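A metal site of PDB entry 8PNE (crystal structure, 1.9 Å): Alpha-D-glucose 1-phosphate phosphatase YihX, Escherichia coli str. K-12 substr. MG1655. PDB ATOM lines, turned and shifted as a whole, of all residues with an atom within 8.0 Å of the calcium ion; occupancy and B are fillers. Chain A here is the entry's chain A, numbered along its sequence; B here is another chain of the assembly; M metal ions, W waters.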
ATOM      1  N   GLN A  79     -22.124  28.345   5.196  1.00  0.00           N
ATOM      2  CA  GLN A  79     -20.858  28.476   4.472  1.00  0.00           C
ATOM      3  C   GLN A  79     -20.981  29.379   3.244  1.00  0.00           C
ATOM      4  O   GLN A  79     -19.965  29.843   2.711  1.00  0.00           O
ATOM      5  CB  GLN A  79     -20.309  27.125   4.035  1.00  0.00           C
ATOM      6  CG  GLN A  79     -18.902  27.183   3.433  1.00  0.00           C
ATOM      7  CD  GLN A  79     -17.841  27.685   4.393  1.00  0.00           C
ATOM      8  OE1 GLN A  79     -17.301  26.952   5.216  1.00  0.00           O
ATOM      9  NE2 GLN A  79     -17.482  28.944   4.224  1.00  0.00           N
ATOM     10  N   ARG A 111     -18.991  32.233  13.438  1.00  0.00           N
ATOM     11  CA  ARG A 111     -18.272  31.113  12.851  1.00  0.00           C
ATOM     12  C   ARG A 111     -18.816  29.870  13.532  1.00  0.00           C
ATOM     13  O   ARG A 111     -19.226  30.012  14.691  1.00  0.00           O
ATOM     14  CB  ARG A 111     -16.768  31.239  13.133  1.00  0.00           C
ATOM     15  CG  ARG A 111     -15.882  30.182  12.501  1.00  0.00           C
ATOM     16  CD  ARG A 111     -14.402  30.304  12.840  1.00  0.00           C
ATOM     17  NE  ARG A 111     -14.108  29.884  14.219  1.00  0.00           N
ATOM     18  CZ  ARG A 111     -13.981  30.710  15.252  1.00  0.00           C
ATOM     19  NH1 ARG A 111     -13.980  30.249  16.467  1.00  0.00           N
ATOM     20  NH2 ARG A 111     -13.951  32.019  15.070  1.00  0.00           N
ATOM     21  N   LEU A 112     -18.889  28.748  12.781  1.00  0.00           N
ATOM     22  CA  LEU A 112     -19.141  27.421  13.339  1.00  0.00           C
ATOM     23  C   LEU A 112     -17.828  26.606  13.282  1.00  0.00           C
ATOM     24  O   LEU A 112     -16.985  26.888  12.440  1.00  0.00           O
ATOM     25  CB  LEU A 112     -20.176  26.718  12.468  1.00  0.00           C
ATOM     26  CG  LEU A 112     -21.433  27.489  12.119  1.00  0.00           C
ATOM     27  CD1 LEU A 112     -22.344  26.666  11.214  1.00  0.00           C
ATOM     28  CD2 LEU A 112     -22.189  27.863  13.379  1.00  0.00           C
ATOM     29  N   HIS A 113     -17.703  25.524  14.063  1.00  0.00           N
ATOM     30  CA  HIS A 113     -16.527  24.683  13.998  1.00  0.00           C
ATOM     31  C   HIS A 113     -16.350  24.040  12.610  1.00  0.00           C
ATOM     32  O   HIS A 113     -15.241  23.625  12.275  1.00  0.00           O
ATOM     33  CB  HIS A 113     -16.512  23.599  15.070  1.00  0.00           C
ATOM     34  CG  HIS A 113     -17.594  22.569  14.950  1.00  0.00           C
ATOM     35  ND1 HIS A 113     -18.910  22.842  15.251  1.00  0.00           N
ATOM     36  CD2 HIS A 113     -17.538  21.254  14.565  1.00  0.00           C
ATOM     37  CE1 HIS A 113     -19.607  21.725  15.084  1.00  0.00           C
ATOM     38  NE2 HIS A 113     -18.795  20.755  14.676  1.00  0.00           N
ATOM     39  N   THR A 114     -17.408  24.015  11.794  1.00  0.00           N
ATOM     40  CA  THR A 114     -17.402  23.355  10.481  1.00  0.00           C
ATOM     41  C   THR A 114     -17.253  24.335   9.328  1.00  0.00           C
ATOM     42  O   THR A 114     -17.275  23.924   8.181  1.00  0.00           O
ATOM     43  CB  THR A 114     -18.703  22.602  10.238  1.00  0.00           C
ATOM     44  OG1 THR A 114     -19.779  23.436  10.675  1.00  0.00           O
ATOM     45  CG2 THR A 114     -18.716  21.271  10.980  1.00  0.00           C
ATOM     46  N   THR A 115     -17.101  25.637   9.586  1.00  0.00           N
ATOM     47  CA  THR A 115     -17.096  26.592   8.478  1.00  0.00           C
ATOM     48  C   THR A 115     -15.768  27.333   8.405  1.00  0.00           C
ATOM     49  O   THR A 115     -15.038  27.445   9.384  1.00  0.00           O
ATOM     50  CB  THR A 115     -18.199  27.652   8.582  1.00  0.00           C
ATOM     51  OG1 THR A 115     -18.040  28.396   9.788  1.00  0.00           O
ATOM     52  CG2 THR A 115     -19.615  27.090   8.473  1.00  0.00           C
ATOM     53  N   PHE A 116     -15.517  27.880   7.195  1.00  0.00           N
ATOM     54  CA  PHE A 116     -14.381  28.731   6.900  1.00  0.00           C
ATOM     55  C   PHE A 116     -14.857  30.178   6.877  1.00  0.00           C
ATOM     56  O   PHE A 116     -15.665  30.539   6.014  1.00  0.00           O
ATOM     57  CB  PHE A 116     -13.750  28.321   5.558  1.00  0.00           C
ATOM     58  CG  PHE A 116     -12.567  29.127   5.094  1.00  0.00           C
ATOM     59  CD1 PHE A 116     -11.491  29.351   5.923  1.00  0.00           C
ATOM     60  CD2 PHE A 116     -12.496  29.586   3.781  1.00  0.00           C
ATOM     61  CE1 PHE A 116     -10.392  30.078   5.488  1.00  0.00           C
ATOM     62  CE2 PHE A 116     -11.398  30.308   3.334  1.00  0.00           C
ATOM     63  CZ  PHE A 116     -10.331  30.524   4.190  1.00  0.00           C
ATOM     64  N   TRP A 117     -14.313  30.986   7.805  1.00  0.00           N
ATOM     65  CA  TRP A 117     -14.867  32.283   8.104  1.00  0.00           C
ATOM     66  C   TRP A 117     -13.825  33.356   7.869  1.00  0.00           C
ATOM     67  O   TRP A 117     -12.622  33.096   7.892  1.00  0.00           O
ATOM     68  CB  TRP A 117     -15.370  32.277   9.555  1.00  0.00           C
ATOM     69  CG  TRP A 117     -16.778  32.777   9.763  1.00  0.00           C
ATOM     70  CD1 TRP A 117     -17.155  33.780  10.614  1.00  0.00           C
ATOM     71  CD2 TRP A 117     -17.983  32.344   9.108  1.00  0.00           C
ATOM     72  NE1 TRP A 117     -18.486  34.017  10.512  1.00  0.00           N
ATOM     73  CE2 TRP A 117     -19.040  33.134   9.637  1.00  0.00           C
ATOM     74  CE3 TRP A 117     -18.296  31.373   8.154  1.00  0.00           C
ATOM     75  CZ2 TRP A 117     -20.364  32.998   9.214  1.00  0.00           C
ATOM     76  CZ3 TRP A 117     -19.616  31.224   7.758  1.00  0.00           C
ATOM     77  CH2 TRP A 117     -20.628  32.053   8.245  1.00  0.00           C
ATOM     78  N   GLU A 119     -12.356  35.579   9.619  1.00  0.00           N
ATOM     79  CA  GLU A 119     -11.270  35.723  10.584  1.00  0.00           C
ATOM     80  C   GLU A 119     -10.214  34.675  10.290  1.00  0.00           C
ATOM     81  O   GLU A 119      -9.062  34.883  10.655  1.00  0.00           O
ATOM     82  CB  GLU A 119     -11.686  35.717  12.058  1.00  0.00           C
ATOM     83  CG  GLU A 119     -12.368  34.441  12.520  1.00  0.00           C
ATOM     84  CD  GLU A 119     -13.875  34.582  12.433  1.00  0.00           C
ATOM     85  OE1 GLU A 119     -14.357  35.470  11.674  1.00  0.00           O
ATOM     86  OE2 GLU A 119     -14.562  33.849  13.175  1.00  0.00           O
ATOM     87  N   GLU A 120     -10.583  33.624   9.545  1.00  0.00           N
ATOM     88  CA  GLU A 120      -9.615  32.576   9.199  1.00  0.00           C
ATOM     89  C   GLU A 120      -8.927  32.908   7.872  1.00  0.00           C
ATOM     90  O   GLU A 120      -8.049  32.217   7.458  1.00  0.00           O
ATOM     91  CB  GLU A 120     -10.304  31.211   9.134  1.00  0.00           C
ATOM     92  CG  GLU A 120     -11.059  30.870  10.400  1.00  0.00           C
ATOM     93  CD  GLU A 120     -11.722  29.492  10.399  1.00  0.00           C
ATOM     94  OE1 GLU A 120     -12.469  29.181   9.437  1.00  0.00           O
ATOM     95  OE2 GLU A 120     -11.447  28.741  11.298  1.00  0.00           O
ATOM     96  N   ARG A 125      -5.705  37.783   8.625  1.00  0.00           N
ATOM     97  CA  ARG A 125      -4.763  37.499   9.675  1.00  0.00           C
ATOM     98  C   ARG A 125      -3.431  38.227   9.462  1.00  0.00           C
ATOM     99  O   ARG A 125      -2.903  38.809  10.423  1.00  0.00           O
ATOM    100  CB  ARG A 125      -4.491  36.018   9.797  1.00  0.00           C
ATOM    101  CG  ARG A 125      -5.707  35.226  10.221  1.00  0.00           C
ATOM    102  CD  ARG A 125      -5.297  33.778  10.257  1.00  0.00           C
ATOM    103  NE  ARG A 125      -6.174  32.949  11.060  1.00  0.00           N
ATOM    104  CZ  ARG A 125      -6.271  31.628  10.926  1.00  0.00           C
ATOM    105  NH1 ARG A 125      -5.585  31.019   9.974  1.00  0.00           N
ATOM    106  NH2 ARG A 125      -7.073  30.931  11.718  1.00  0.00           N
ATOM    107  N   GLY B  21      -9.285  27.406   0.106  1.00  0.00           N
ATOM    108  CA  GLY B  21      -9.213  27.905   1.474  1.00  0.00           C
ATOM    109  C   GLY B  21     -10.095  27.116   2.429  1.00  0.00           C
ATOM    110  O   GLY B  21      -9.683  26.766   3.528  1.00  0.00           O
ATOM    111  N   ALA B  22     -11.310  26.792   1.984  1.00  0.00           N
ATOM    112  CA  ALA B  22     -12.239  26.112   2.856  1.00  0.00           C
ATOM    113  C   ALA B  22     -11.820  24.670   3.049  1.00  0.00           C
ATOM    114  O   ALA B  22     -11.916  24.107   4.145  1.00  0.00           O
ATOM    115  CB  ALA B  22     -13.622  26.222   2.269  1.00  0.00           C
ATOM    116  N   SER B  24      -8.747  23.650   2.847  1.00  0.00           N
ATOM    117  CA  SER B  24      -7.552  23.764   3.662  1.00  0.00           C
ATOM    118  C   SER B  24      -7.955  23.908   5.131  1.00  0.00           C
ATOM    119  O   SER B  24      -7.346  23.282   6.014  1.00  0.00           O
ATOM    120  CB  SER B  24      -6.655  24.899   3.219  1.00  0.00           C
ATOM    121  OG  SER B  24      -5.483  25.037   4.027  1.00  0.00           O
ATOM    122  N   ASP B  25      -8.983  24.727   5.366  1.00  0.00           N
ATOM    123  CA  ASP B  25      -9.499  24.977   6.705  1.00  0.00           C
ATOM    124  C   ASP B  25      -9.897  23.649   7.368  1.00  0.00           C
ATOM    125  O   ASP B  25      -9.549  23.367   8.515  1.00  0.00           O
ATOM    126  CB  ASP B  25     -10.652  25.978   6.632  1.00  0.00           C
ATOM    127  CG  ASP B  25     -11.366  26.254   7.948  1.00  0.00           C
ATOM    128  OD1 ASP B  25     -10.703  26.607   8.940  1.00  0.00           O
ATOM    129  OD2 ASP B  25     -12.582  26.173   7.973  1.00  0.00           O
ATOM    130  N   LEU B  26     -10.637  22.839   6.648  1.00  0.00           N
ATOM    131  CA  LEU B  26     -11.100  21.572   7.179  1.00  0.00           C
ATOM    132  C   LEU B  26      -9.976  20.539   7.291  1.00  0.00           C
ATOM    133  O   LEU B  26      -9.875  19.883   8.298  1.00  0.00           O
ATOM    134  CB  LEU B  26     -12.194  21.051   6.259  1.00  0.00           C
ATOM    135  CG  LEU B  26     -12.783  19.711   6.700  1.00  0.00           C
ATOM    136  CD1 LEU B  26     -13.131  19.716   8.186  1.00  0.00           C
ATOM    137  CD2 LEU B  26     -14.026  19.391   5.891  1.00  0.00           C
ATOM    138  N   ARG B  28      -6.606  20.854   6.933  1.00  0.00           N
ATOM    139  CA  ARG B  28      -5.319  21.361   7.408  1.00  0.00           C
ATOM    140  C   ARG B  28      -4.219  21.157   6.357  1.00  0.00           C
ATOM    141  O   ARG B  28      -3.035  21.343   6.659  1.00  0.00           O
ATOM    142  CB  ARG B  28      -4.904  20.713   8.727  1.00  0.00           C
ATOM    143  CG  ARG B  28      -5.985  20.628   9.781  1.00  0.00           C
ATOM    144  CD  ARG B  28      -5.942  21.871  10.625  1.00  0.00           C
ATOM    145  NE  ARG B  28      -6.780  22.913  10.067  1.00  0.00           N
ATOM    146  CZ  ARG B  28      -6.676  24.199  10.366  1.00  0.00           C
ATOM    147  NH1 ARG B  28      -5.615  24.641  11.014  1.00  0.00           N
ATOM    148  NH2 ARG B  28      -7.628  25.038   9.979  1.00  0.00           N
HETATM  149 CA    CA M   1     -12.819  27.001  10.283  1.00  0.00          CA
HETATM  150  O   HOH W   1     -13.616  24.767  10.490  1.00  0.00           O
HETATM  151  O   HOH W   2     -11.408  25.798  11.762  1.00  0.00           O
HETATM  152  O   HOH W   3     -14.121  27.088  12.353  1.00  0.00           O
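OE1 of Glu 120 lies close to N of Trp 117 (3.1 Å). The side-chain hydroxyl (OG1) of Thr 115 sits at hydrogen-bond distance from the backbone NH (N) of Leu 112. The side-chain carboxylate of Asp 25 of chain B lies close to the backbone NH of Phe 116, 3.5 Å away. NH2 of Arg 28 of chain B is in hydrogen-bond range of O of Asp 25 of chain B.
Of the 17 residues printed, 3 come within 4 Å of the calcium ion.
The calcium ion is bound by OE1 of Glu 120 (2.4 Å). The calcium ion is bound by water W2. Water W1 is bound to the calcium ion, at 2.4 Å. The calcium ion is bound by O of Thr 115. The calcium ion is bound by OE2 of Glu 120 (2.4 Å). The calcium ion is bound by water W3 (2.4 Å). OD2 of Asp 25 of chain B is bound to the calcium ion (2.5 Å). OD1 of Asp 25 of chain B binds the calcium ion, 2.5 Å away. The calcium ion has eight donor atoms within binding distance.
Water W3 lies within hydrogen-bond range of the backbone carbonyl oxygen of Leu 112 (2.9 Å) and the guanidinium group of Arg 111 (3.4 Å).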
